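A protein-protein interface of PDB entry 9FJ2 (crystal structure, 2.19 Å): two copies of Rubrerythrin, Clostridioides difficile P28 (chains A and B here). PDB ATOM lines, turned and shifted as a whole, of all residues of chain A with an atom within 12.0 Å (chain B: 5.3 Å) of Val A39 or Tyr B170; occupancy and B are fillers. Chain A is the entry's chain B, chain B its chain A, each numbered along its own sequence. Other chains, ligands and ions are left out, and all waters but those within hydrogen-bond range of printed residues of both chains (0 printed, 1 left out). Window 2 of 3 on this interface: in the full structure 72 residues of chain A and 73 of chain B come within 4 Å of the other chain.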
ATOM      1  N   TYR A  26      -3.081  -1.276 -26.202  1.00  0.00           N
ATOM      2  CA  TYR A  26      -3.169  -1.476 -24.761  1.00  0.00           C
ATOM      3  C   TYR A  26      -1.950  -2.180 -24.184  1.00  0.00           C
ATOM      4  O   TYR A  26      -1.760  -2.152 -22.962  1.00  0.00           O
ATOM      5  CB  TYR A  26      -4.442  -2.253 -24.426  1.00  0.00           C
ATOM      6  CG  TYR A  26      -5.695  -1.534 -24.866  1.00  0.00           C
ATOM      7  CD1 TYR A  26      -5.722  -0.149 -24.946  1.00  0.00           C
ATOM      8  CD2 TYR A  26      -6.846  -2.233 -25.205  1.00  0.00           C
ATOM      9  CE1 TYR A  26      -6.854   0.522 -25.348  1.00  0.00           C
ATOM     10  CE2 TYR A  26      -7.990  -1.568 -25.608  1.00  0.00           C
ATOM     11  CZ  TYR A  26      -7.984  -0.189 -25.677  1.00  0.00           C
ATOM     12  OH  TYR A  26      -9.108   0.492 -26.075  1.00  0.00           O
ATOM     13  N   THR A  27      -1.121  -2.805 -25.022  1.00  0.00           N
ATOM     14  CA  THR A  27       0.132  -3.361 -24.530  1.00  0.00           C
ATOM     15  C   THR A  27       1.185  -2.278 -24.335  1.00  0.00           C
ATOM     16  O   THR A  27       2.012  -2.380 -23.422  1.00  0.00           O
ATOM     17  CB  THR A  27       0.652  -4.439 -25.481  1.00  0.00           C
ATOM     18  OG1 THR A  27       0.494  -4.003 -26.837  1.00  0.00           O
ATOM     19  CG2 THR A  27      -0.115  -5.739 -25.277  1.00  0.00           C
ATOM     20  N   TYR A  28       1.170  -1.238 -25.173  1.00  0.00           N
ATOM     21  CA  TYR A  28       2.047  -0.096 -24.940  1.00  0.00           C
ATOM     22  C   TYR A  28       1.538   0.750 -23.782  1.00  0.00           C
ATOM     23  O   TYR A  28       2.333   1.285 -23.000  1.00  0.00           O
ATOM     24  CB  TYR A  28       2.166   0.758 -26.203  1.00  0.00           C
ATOM     25  CG  TYR A  28       2.416  -0.008 -27.482  1.00  0.00           C
ATOM     26  CD1 TYR A  28       3.244  -1.124 -27.503  1.00  0.00           C
ATOM     27  CD2 TYR A  28       1.832   0.397 -28.675  1.00  0.00           C
ATOM     28  CE1 TYR A  28       3.473  -1.820 -28.678  1.00  0.00           C
ATOM     29  CE2 TYR A  28       2.054  -0.291 -29.851  1.00  0.00           C
ATOM     30  CZ  TYR A  28       2.875  -1.397 -29.846  1.00  0.00           C
ATOM     31  OH  TYR A  28       3.095  -2.080 -31.019  1.00  0.00           O
ATOM     32  N   TYR A  29       0.214   0.889 -23.660  1.00  0.00           N
ATOM     33  CA  TYR A  29      -0.355   1.642 -22.548  1.00  0.00           C
ATOM     34  C   TYR A  29      -0.050   0.969 -21.217  1.00  0.00           C
ATOM     35  O   TYR A  29       0.186   1.646 -20.209  1.00  0.00           O
ATOM     36  CB  TYR A  29      -1.865   1.800 -22.732  1.00  0.00           C
ATOM     37  CG  TYR A  29      -2.256   2.709 -23.876  1.00  0.00           C
ATOM     38  CD1 TYR A  29      -1.374   3.667 -24.357  1.00  0.00           C
ATOM     39  CD2 TYR A  29      -3.509   2.617 -24.467  1.00  0.00           C
ATOM     40  CE1 TYR A  29      -1.725   4.504 -25.397  1.00  0.00           C
ATOM     41  CE2 TYR A  29      -3.871   3.452 -25.510  1.00  0.00           C
ATOM     42  CZ  TYR A  29      -2.974   4.393 -25.970  1.00  0.00           C
ATOM     43  OH  TYR A  29      -3.324   5.227 -27.006  1.00  0.00           O
ATOM     44  N   ALA A  30      -0.053  -0.366 -21.194  1.00  0.00           N
ATOM     45  CA  ALA A  30       0.281  -1.087 -19.970  1.00  0.00           C
ATOM     46  C   ALA A  30       1.721  -0.823 -19.550  1.00  0.00           C
ATOM     47  O   ALA A  30       2.005  -0.627 -18.362  1.00  0.00           O
ATOM     48  CB  ALA A  30       0.042  -2.583 -20.161  1.00  0.00           C
ATOM     49  N   SER A  31       2.648  -0.813 -20.511  1.00  0.00           N
ATOM     50  CA  SER A  31       4.042  -0.535 -20.183  1.00  0.00           C
ATOM     51  C   SER A  31       4.226   0.910 -19.737  1.00  0.00           C
ATOM     52  O   SER A  31       5.005   1.187 -18.817  1.00  0.00           O
ATOM     53  CB  SER A  31       4.936  -0.844 -21.383  1.00  0.00           C
ATOM     54  OG  SER A  31       6.279  -0.479 -21.120  1.00  0.00           O
ATOM     55  N   LYS A  32       3.519   1.845 -20.377  1.00  0.00           N
ATOM     56  CA  LYS A  32       3.624   3.249 -19.991  1.00  0.00           C
ATOM     57  C   LYS A  32       3.036   3.486 -18.606  1.00  0.00           C
ATOM     58  O   LYS A  32       3.557   4.301 -17.836  1.00  0.00           O
ATOM     59  CB  LYS A  32       2.930   4.127 -21.031  1.00  0.00           C
ATOM     60  CG  LYS A  32       2.960   5.612 -20.716  1.00  0.00           C
ATOM     61  CD  LYS A  32       4.383   6.127 -20.568  1.00  0.00           C
ATOM     62  CE  LYS A  32       4.407   7.445 -19.809  1.00  0.00           C
ATOM     63  NZ  LYS A  32       5.499   8.347 -20.263  1.00  0.00           N
ATOM     64  N   ALA A  33       1.952   2.784 -18.271  1.00  0.00           N
ATOM     65  CA  ALA A  33       1.362   2.931 -16.944  1.00  0.00           C
ATOM     66  C   ALA A  33       2.257   2.320 -15.875  1.00  0.00           C
ATOM     67  O   ALA A  33       2.380   2.866 -14.774  1.00  0.00           O
ATOM     68  CB  ALA A  33      -0.025   2.291 -16.904  1.00  0.00           C
ATOM     69  N   LYS A  34       2.891   1.185 -16.175  1.00  0.00           N
ATOM     70  CA  LYS A  34       3.759   0.563 -15.182  1.00  0.00           C
ATOM     71  C   LYS A  34       4.972   1.442 -14.901  1.00  0.00           C
ATOM     72  O   LYS A  34       5.526   1.410 -13.796  1.00  0.00           O
ATOM     73  CB  LYS A  34       4.174  -0.835 -15.665  1.00  0.00           C
ATOM     74  CG  LYS A  34       4.940  -1.722 -14.666  1.00  0.00           C
ATOM     75  CD  LYS A  34       4.007  -2.122 -13.517  1.00  0.00           C
ATOM     76  CE  LYS A  34       4.694  -3.037 -12.520  1.00  0.00           C
ATOM     77  NZ  LYS A  34       5.103  -4.370 -13.076  1.00  0.00           N
ATOM     78  N   LYS A  35       5.388   2.237 -15.890  1.00  0.00           N
ATOM     79  CA  LYS A  35       6.471   3.197 -15.708  1.00  0.00           C
ATOM     80  C   LYS A  35       5.991   4.479 -15.040  1.00  0.00           C
ATOM     81  O   LYS A  35       6.788   5.172 -14.399  1.00  0.00           O
ATOM     82  CB  LYS A  35       7.116   3.540 -17.054  1.00  0.00           C
ATOM     83  CG  LYS A  35       8.118   2.514 -17.557  1.00  0.00           C
ATOM     84  CD  LYS A  35       9.316   2.400 -16.631  1.00  0.00           C
ATOM     85  CE  LYS A  35      10.301   1.362 -17.144  1.00  0.00           C
ATOM     86  NZ  LYS A  35      11.555   1.342 -16.344  1.00  0.00           N
ATOM     87  N   ASP A  36       4.708   4.817 -15.186  1.00  0.00           N
ATOM     88  CA  ASP A  36       4.163   6.032 -14.590  1.00  0.00           C
ATOM     89  C   ASP A  36       3.803   5.866 -13.120  1.00  0.00           C
ATOM     90  O   ASP A  36       3.445   6.856 -12.471  1.00  0.00           O
ATOM     91  CB  ASP A  36       2.923   6.489 -15.366  1.00  0.00           C
ATOM     92  CG  ASP A  36       3.256   7.459 -16.482  1.00  0.00           C
ATOM     93  OD1 ASP A  36       4.420   7.904 -16.560  1.00  0.00           O
ATOM     94  OD2 ASP A  36       2.352   7.776 -17.283  1.00  0.00           O
ATOM     95  N   GLY A  37       3.882   4.654 -12.587  1.00  0.00           N
ATOM     96  CA  GLY A  37       3.553   4.397 -11.206  1.00  0.00           C
ATOM     97  C   GLY A  37       2.157   3.873 -10.953  1.00  0.00           C
ATOM     98  O   GLY A  37       1.584   4.178  -9.901  1.00  0.00           O
ATOM     99  N   TYR A  38       1.593   3.092 -11.876  1.00  0.00           N
ATOM    100  CA  TYR A  38       0.235   2.555 -11.741  1.00  0.00           C
ATOM    101  C   TYR A  38       0.273   1.087 -12.161  1.00  0.00           C
ATOM    102  O   TYR A  38       0.099   0.766 -13.339  1.00  0.00           O
ATOM    103  CB  TYR A  38      -0.760   3.347 -12.578  1.00  0.00           C
ATOM    104  CG  TYR A  38      -0.659   4.848 -12.432  1.00  0.00           C
ATOM    105  CD1 TYR A  38      -1.100   5.487 -11.280  1.00  0.00           C
ATOM    106  CD2 TYR A  38      -0.134   5.630 -13.454  1.00  0.00           C
ATOM    107  CE1 TYR A  38      -1.015   6.861 -11.147  1.00  0.00           C
ATOM    108  CE2 TYR A  38      -0.045   7.004 -13.331  1.00  0.00           C
ATOM    109  CZ  TYR A  38      -0.488   7.614 -12.175  1.00  0.00           C
ATOM    110  OH  TYR A  38      -0.401   8.982 -12.049  1.00  0.00           O
ATOM    111  N   VAL A  39       0.495   0.199 -11.189  1.00  0.00           N
ATOM    112  CA  VAL A  39       0.572  -1.225 -11.499  1.00  0.00           C
ATOM    113  C   VAL A  39      -0.812  -1.784 -11.807  1.00  0.00           C
ATOM    114  O   VAL A  39      -0.978  -2.594 -12.727  1.00  0.00           O
ATOM    115  CB  VAL A  39       1.249  -1.989 -10.347  1.00  0.00           C
ATOM    116  CG1 VAL A  39       1.235  -3.489 -10.613  1.00  0.00           C
ATOM    117  CG2 VAL A  39       2.668  -1.490 -10.149  1.00  0.00           C
ATOM    118  N   GLN A  40      -1.828  -1.363 -11.047  1.00  0.00           N
ATOM    119  CA  GLN A  40      -3.182  -1.844 -11.303  1.00  0.00           C
ATOM    120  C   GLN A  40      -3.700  -1.352 -12.648  1.00  0.00           C
ATOM    121  O   GLN A  40      -4.300  -2.124 -13.407  1.00  0.00           O
ATOM    122  CB  GLN A  40      -4.127  -1.412 -10.182  1.00  0.00           C
ATOM    123  CG  GLN A  40      -5.542  -1.944 -10.359  1.00  0.00           C
ATOM    124  CD  GLN A  40      -6.549  -1.290  -9.432  1.00  0.00           C
ATOM    125  OE1 GLN A  40      -6.376  -0.148  -9.008  1.00  0.00           O
ATOM    126  NE2 GLN A  40      -7.612  -2.019  -9.113  1.00  0.00           N
ATOM    127  N   ILE A  41      -3.486  -0.072 -12.958  1.00  0.00           N
ATOM    128  CA  ILE A  41      -3.903   0.456 -14.254  1.00  0.00           C
ATOM    129  C   ILE A  41      -3.143  -0.239 -15.377  1.00  0.00           C
ATOM    130  O   ILE A  41      -3.703  -0.524 -16.443  1.00  0.00           O
ATOM    131  CB  ILE A  41      -3.717   1.985 -14.294  1.00  0.00           C
ATOM    132  CG1 ILE A  41      -4.634   2.655 -13.267  1.00  0.00           C
ATOM    133  CG2 ILE A  41      -3.992   2.529 -15.688  1.00  0.00           C
ATOM    134  CD1 ILE A  41      -4.301   4.106 -12.998  1.00  0.00           C
ATOM    135  N   SER A  42      -1.861  -0.538 -15.149  1.00  0.00           N
ATOM    136  CA  SER A  42      -1.097  -1.301 -16.130  1.00  0.00           C
ATOM    137  C   SER A  42      -1.659  -2.707 -16.295  1.00  0.00           C
ATOM    138  O   SER A  42      -1.665  -3.256 -17.402  1.00  0.00           O
ATOM    139  CB  SER A  42       0.374  -1.363 -15.720  1.00  0.00           C
ATOM    140  OG  SER A  42       1.095  -2.260 -16.546  1.00  0.00           O
ATOM    141  N   ASN A  43      -2.140  -3.306 -15.202  1.00  0.00           N
ATOM    142  CA  ASN A  43      -2.728  -4.638 -15.293  1.00  0.00           C
ATOM    143  C   ASN A  43      -4.070  -4.598 -16.012  1.00  0.00           C
ATOM    144  O   ASN A  43      -4.414  -5.529 -16.751  1.00  0.00           O
ATOM    145  CB  ASN A  43      -2.885  -5.242 -13.898  1.00  0.00           C
ATOM    146  CG  ASN A  43      -1.556  -5.526 -13.232  1.00  0.00           C
ATOM    147  OD1 ASN A  43      -0.584  -5.898 -13.891  1.00  0.00           O
ATOM    148  ND2 ASN A  43      -1.506  -5.348 -11.918  1.00  0.00           N
ATOM    149  N   ILE A  44      -4.843  -3.529 -15.807  1.00  0.00           N
ATOM    150  CA  ILE A  44      -6.126  -3.400 -16.489  1.00  0.00           C
ATOM    151  C   ILE A  44      -5.913  -3.237 -17.989  1.00  0.00           C
ATOM    152  O   ILE A  44      -6.651  -3.808 -18.801  1.00  0.00           O
ATOM    153  CB  ILE A  44      -6.929  -2.231 -15.889  1.00  0.00           C
ATOM    154  CG1 ILE A  44      -7.551  -2.649 -14.555  1.00  0.00           C
ATOM    155  CG2 ILE A  44      -8.012  -1.765 -16.852  1.00  0.00           C
ATOM    156  CD1 ILE A  44      -7.726  -1.511 -13.577  1.00  0.00           C
ATOM    157  N   PHE A  45      -4.894  -2.470 -18.382  1.00  0.00           N
ATOM    158  CA  PHE A  45      -4.555  -2.357 -19.796  1.00  0.00           C
ATOM    159  C   PHE A  45      -4.163  -3.704 -20.389  1.00  0.00           C
ATOM    160  O   PHE A  45      -4.444  -3.970 -21.563  1.00  0.00           O
ATOM    161  CB  PHE A  45      -3.419  -1.353 -19.987  1.00  0.00           C
ATOM    162  CG  PHE A  45      -3.878   0.071 -20.103  1.00  0.00           C
ATOM    163  CD1 PHE A  45      -4.929   0.408 -20.938  1.00  0.00           C
ATOM    164  CD2 PHE A  45      -3.253   1.074 -19.382  1.00  0.00           C
ATOM    165  CE1 PHE A  45      -5.352   1.719 -21.049  1.00  0.00           C
ATOM    166  CE2 PHE A  45      -3.671   2.388 -19.487  1.00  0.00           C
ATOM    167  CZ  PHE A  45      -4.721   2.710 -20.324  1.00  0.00           C
ATOM    168  N   GLU A  46      -3.527  -4.570 -19.595  1.00  0.00           N
ATOM    169  CA  GLU A  46      -3.025  -5.833 -20.128  1.00  0.00           C
ATOM    170  C   GLU A  46      -4.162  -6.806 -20.425  1.00  0.00           C
ATOM    171  O   GLU A  46      -4.256  -7.342 -21.536  1.00  0.00           O
ATOM    172  CB  GLU A  46      -2.019  -6.452 -19.159  1.00  0.00           C
ATOM    173  CG  GLU A  46      -1.342  -7.709 -19.691  1.00  0.00           C
ATOM    174  CD  GLU A  46      -0.280  -7.407 -20.735  1.00  0.00           C
ATOM    175  OE1 GLU A  46      -0.343  -7.996 -21.836  1.00  0.00           O
ATOM    176  OE2 GLU A  46       0.616  -6.582 -20.456  1.00  0.00           O
ATOM    177  N   GLN A  47      -5.037  -7.054 -19.447  1.00  0.00           N
ATOM    178  CA  GLN A  47      -6.114  -8.010 -19.682  1.00  0.00           C
ATOM    179  C   GLN A  47      -7.131  -7.492 -20.690  1.00  0.00           C
ATOM    180  O   GLN A  47      -7.804  -8.298 -21.343  1.00  0.00           O
ATOM    181  CB  GLN A  47      -6.819  -8.380 -18.375  1.00  0.00           C
ATOM    182  CG  GLN A  47      -7.628  -7.269 -17.732  1.00  0.00           C
ATOM    183  CD  GLN A  47      -8.567  -7.794 -16.662  1.00  0.00           C
ATOM    184  OE1 GLN A  47      -8.722  -9.005 -16.497  1.00  0.00           O
ATOM    185  NE2 GLN A  47      -9.201  -6.885 -15.931  1.00  0.00           N
ATOM    186  N   THR A  48      -7.257  -6.170 -20.836  1.00  0.00           N
ATOM    187  CA  THR A  48      -8.101  -5.631 -21.898  1.00  0.00           C
ATOM    188  C   THR A  48      -7.530  -5.972 -23.269  1.00  0.00           C
ATOM    189  O   THR A  48      -8.278  -6.333 -24.185  1.00  0.00           O
ATOM    190  CB  THR A  48      -8.251  -4.118 -21.742  1.00  0.00           C
ATOM    191  OG1 THR A  48      -8.688  -3.810 -20.413  1.00  0.00           O
ATOM    192  CG2 THR A  48      -9.267  -3.583 -22.737  1.00  0.00           C
ATOM    193  N   GLU B 144      -3.850  -3.732  -1.005  1.00  0.00           N
ATOM    194  CA  GLU B 144      -3.054  -4.935  -1.211  1.00  0.00           C
ATOM    195  C   GLU B 144      -1.836  -4.596  -2.056  1.00  0.00           C
ATOM    196  O   GLU B 144      -1.955  -3.910  -3.076  1.00  0.00           O
ATOM    197  CB  GLU B 144      -3.877  -6.035  -1.888  1.00  0.00           C
ATOM    198  CG  GLU B 144      -3.043  -7.191  -2.421  1.00  0.00           C
ATOM    199  CD  GLU B 144      -3.888  -8.364  -2.877  1.00  0.00           C
ATOM    200  OE1 GLU B 144      -5.099  -8.381  -2.571  1.00  0.00           O
ATOM    201  OE2 GLU B 144      -3.341  -9.274  -3.534  1.00  0.00           O
ATOM    202  N   CYS B 145      -0.669  -5.080  -1.630  1.00  0.00           N
ATOM    203  CA  CYS B 145       0.566  -4.907  -2.387  1.00  0.00           C
ATOM    204  C   CYS B 145       0.614  -5.957  -3.491  1.00  0.00           C
ATOM    205  O   CYS B 145       0.702  -7.157  -3.213  1.00  0.00           O
ATOM    206  CB  CYS B 145       1.776  -5.018  -1.462  1.00  0.00           C
ATOM    207  SG  CYS B 145       3.377  -4.885  -2.290  1.00  0.00           S
ATOM    208  N   LEU B 146       0.563  -5.508  -4.746  1.00  0.00           N
ATOM    209  CA  LEU B 146       0.512  -6.425  -5.882  1.00  0.00           C
ATOM    210  C   LEU B 146       1.835  -7.138  -6.140  1.00  0.00           C
ATOM    211  O   LEU B 146       1.917  -7.916  -7.096  1.00  0.00           O
ATOM    212  CB  LEU B 146       0.074  -5.672  -7.140  1.00  0.00           C
ATOM    213  CG  LEU B 146      -1.390  -5.223  -7.182  1.00  0.00           C
ATOM    214  CD1 LEU B 146      -1.587  -4.093  -8.181  1.00  0.00           C
ATOM    215  CD2 LEU B 146      -2.307  -6.395  -7.504  1.00  0.00           C
ATOM    216  N   ASN B 147       2.863  -6.900  -5.327  1.00  0.00           N
ATOM    217  CA  ASN B 147       4.150  -7.567  -5.489  1.00  0.00           C
ATOM    218  C   ASN B 147       4.353  -8.693  -4.483  1.00  0.00           C
ATOM    219  O   ASN B 147       4.707  -9.811  -4.870  1.00  0.00           O
ATOM    220  CB  ASN B 147       5.290  -6.548  -5.372  1.00  0.00           C
ATOM    221  CG  ASN B 147       6.654  -7.177  -5.583  1.00  0.00           C
ATOM    222  OD1 ASN B 147       7.383  -7.444  -4.627  1.00  0.00           O
ATOM    223  ND2 ASN B 147       7.005  -7.420  -6.840  1.00  0.00           N
ATOM    224  N   HIS B 166       8.500  -2.102  -1.790  1.00  0.00           N
ATOM    225  CA  HIS B 166       8.100  -1.672  -3.122  1.00  0.00           C
ATOM    226  C   HIS B 166       7.261  -0.397  -3.036  1.00  0.00           C
ATOM    227  O   HIS B 166       6.558  -0.178  -2.045  1.00  0.00           O
ATOM    228  CB  HIS B 166       7.303  -2.767  -3.840  1.00  0.00           C
ATOM    229  CG  HIS B 166       8.160  -3.756  -4.571  1.00  0.00           C
ATOM    230  ND1 HIS B 166       9.059  -4.580  -3.929  1.00  0.00           N
ATOM    231  CD2 HIS B 166       8.254  -4.051  -5.889  1.00  0.00           C
ATOM    232  CE1 HIS B 166       9.672  -5.339  -4.820  1.00  0.00           C
ATOM    233  NE2 HIS B 166       9.200  -5.039  -6.017  1.00  0.00           N
ATOM    234  N   PRO B 167       7.317   0.475  -4.056  1.00  0.00           N
ATOM    235  CA  PRO B 167       6.598   1.756  -3.970  1.00  0.00           C
ATOM    236  C   PRO B 167       5.084   1.610  -3.997  1.00  0.00           C
ATOM    237  O   PRO B 167       4.555   0.496  -4.076  1.00  0.00           O
ATOM    238  CB  PRO B 167       7.107   2.527  -5.194  1.00  0.00           C
ATOM    239  CG  PRO B 167       7.576   1.475  -6.142  1.00  0.00           C
ATOM    240  CD  PRO B 167       8.115   0.366  -5.289  1.00  0.00           C
ATOM    241  N   ARG B 168       4.377   2.743  -3.933  1.00  0.00           N
ATOM    242  CA  ARG B 168       2.917   2.729  -3.907  1.00  0.00           C
ATOM    243  C   ARG B 168       2.303   2.246  -5.210  1.00  0.00           C
ATOM    244  O   ARG B 168       1.123   1.879  -5.217  1.00  0.00           O
ATOM    245  CB  ARG B 168       2.369   4.120  -3.595  1.00  0.00           C
ATOM    246  CG  ARG B 168       2.096   4.345  -2.134  1.00  0.00           C
ATOM    247  CD  ARG B 168       1.072   5.432  -1.910  1.00  0.00           C
ATOM    248  NE  ARG B 168       1.428   6.670  -2.588  1.00  0.00           N
ATOM    249  CZ  ARG B 168       1.656   7.817  -1.959  1.00  0.00           C
ATOM    250  NH1 ARG B 168       1.571   7.875  -0.637  1.00  0.00           N
ATOM    251  NH2 ARG B 168       1.974   8.902  -2.649  1.00  0.00           N
ATOM    252  N   SER B 169       3.066   2.257  -6.305  1.00  0.00           N
ATOM    253  CA  SER B 169       2.533   1.811  -7.588  1.00  0.00           C
ATOM    254  C   SER B 169       1.918   0.422  -7.481  1.00  0.00           C
ATOM    255  O   SER B 169       0.868   0.153  -8.074  1.00  0.00           O
ATOM    256  CB  SER B 169       3.636   1.838  -8.646  1.00  0.00           C
ATOM    257  OG  SER B 169       4.698   0.966  -8.303  1.00  0.00           O
ATOM    258  N   TYR B 170       2.538  -0.460  -6.698  1.00  0.00           N
ATOM    259  CA  TYR B 170       2.089  -1.839  -6.549  1.00  0.00           C
ATOM    260  C   TYR B 170       0.916  -1.991  -5.587  1.00  0.00           C
ATOM    261  O   TYR B 170       0.576  -3.125  -5.231  1.00  0.00           O
ATOM    262  CB  TYR B 170       3.250  -2.723  -6.083  1.00  0.00           C
ATOM    263  CG  TYR B 170       4.365  -2.863  -7.096  1.00  0.00           C
ATOM    264  CD1 TYR B 170       5.300  -1.852  -7.275  1.00  0.00           C
ATOM    265  CD2 TYR B 170       4.482  -4.008  -7.874  1.00  0.00           C
ATOM    266  CE1 TYR B 170       6.318  -1.975  -8.200  1.00  0.00           C
ATOM    267  CE2 TYR B 170       5.498  -4.140  -8.803  1.00  0.00           C
ATOM    268  CZ  TYR B 170       6.413  -3.121  -8.961  1.00  0.00           C
ATOM    269  OH  TYR B 170       7.427  -3.244  -9.882  1.00  0.00           O
ATOM    270  N   PHE B 171       0.289  -0.900  -5.158  1.00  0.00           N
ATOM    271  CA  PHE B 171      -0.817  -0.961  -4.214  1.00  0.00           C
ATOM    272  C   PHE B 171      -2.140  -0.724  -4.930  1.00  0.00           C
ATOM    273  O   PHE B 171      -2.235   0.126  -5.821  1.00  0.00           O
ATOM    274  CB  PHE B 171      -0.636   0.063  -3.093  1.00  0.00           C
ATOM    275  CG  PHE B 171       0.253  -0.412  -1.982  1.00  0.00           C
ATOM    276  CD1 PHE B 171      -0.193  -1.366  -1.081  1.00  0.00           C
ATOM    277  CD2 PHE B 171       1.536   0.089  -1.841  1.00  0.00           C
ATOM    278  CE1 PHE B 171       0.625  -1.810  -0.059  1.00  0.00           C
ATOM    279  CE2 PHE B 171       2.359  -0.347  -0.819  1.00  0.00           C
ATOM    280  CZ  PHE B 171       1.903  -1.298   0.072  1.00  0.00           C
ATOM    281  N   GLU B 172      -3.160  -1.483  -4.532  1.00  0.00           N
ATOM    282  CA  GLU B 172      -4.469  -1.414  -5.161  1.00  0.00           C
ATOM    283  C   GLU B 172      -5.541  -1.710  -4.123  1.00  0.00           C
ATOM    284  O   GLU B 172      -5.271  -2.290  -3.068  1.00  0.00           O
ATOM    285  CB  GLU B 172      -4.590  -2.400  -6.330  1.00  0.00           C
ATOM    286  CG  GLU B 172      -4.829  -3.841  -5.889  1.00  0.00           C
ATOM    287  CD  GLU B 172      -5.420  -4.708  -6.986  1.00  0.00           C
ATOM    288  OE1 GLU B 172      -5.660  -4.191  -8.096  1.00  0.00           O
ATOM    289  OE2 GLU B 172      -5.642  -5.912  -6.738  1.00  0.00           O
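The backbone carbonyl oxygen (O) of Ser B169 lies within hydrogen-bond range of the backbone NH (N) of Val A39, at 3.1 Å.
The side-chain carboxylate of Glu B172 sits at hydrogen-bond distance from the side-chain amide nitrogen of Gln A40 (3.1 Å).
The backbone NH (N) of Glu B144 lies within hydrogen-bond range of the backbone carbonyl oxygen (O) of Glu B172, 2.9 Å away.
The backbone carbonyl oxygen (O) of Tyr B170 lies within hydrogen-bond range of the backbone NH (N) of Leu B146 (2.4 Å).
ND2 of Asn A43 sits at hydrogen-bond distance from O of Val A39 (2.9 Å).
Among the printed residues, pairs that only touch across the chains: Lys A34 with Tyr B170, Gly A37 with Ser B169, Val A39 with Leu B146, Val A39 with Tyr B170, Gln A40 with Leu B146 and Asn A43 with Leu B146.
Tyr B170 touches just these residues of chain A: Lys A34 and Val A39.
No residue of chain A comes within 4 Å of Cys B145.
Leu B146 touches just these residues of chain A: Val A39, Gln A40 and Asn A43.
No residue of chain A comes within 4 Å of Asn B147.
No residue of chain A comes within 4 Å of His B166.
No residue of chain A comes within 4 Å of Pro B167.
Glu B172 touches just one residue of chain A: Gln A40 (3.1 Å).
Of the printed residues of chain B, Lys A34 touches Tyr B170.
Printed residues of chain B within 4 Å of Asn A43: Leu B146 (3.9 Å).
Printed residues of chain B within 4 Å of Gln A40: Leu B146 and Glu B172.
Of the printed residues of chain B, Gly A37 touches Ser B169.
Arg B168 touches none of the printed residues of chain A.
Of the 11 printed residues of chain B, 4 touch a printed residue of chain A.
Printed residues of chain A that touch a printed residue of chain B: Lys A34, Gly A37, Val A39, Gln A40 and Asn A43.
Hydrophobic or aromatic side chains of chain A that line the printed part of chain B: Val A39.
Among the printed residues, 8 pairs touch across the chains.
No position is printed for both chains.
Of the 8 pairs that touch across the chains among the printed residues, none has its exchanged pair printed and touching as well.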
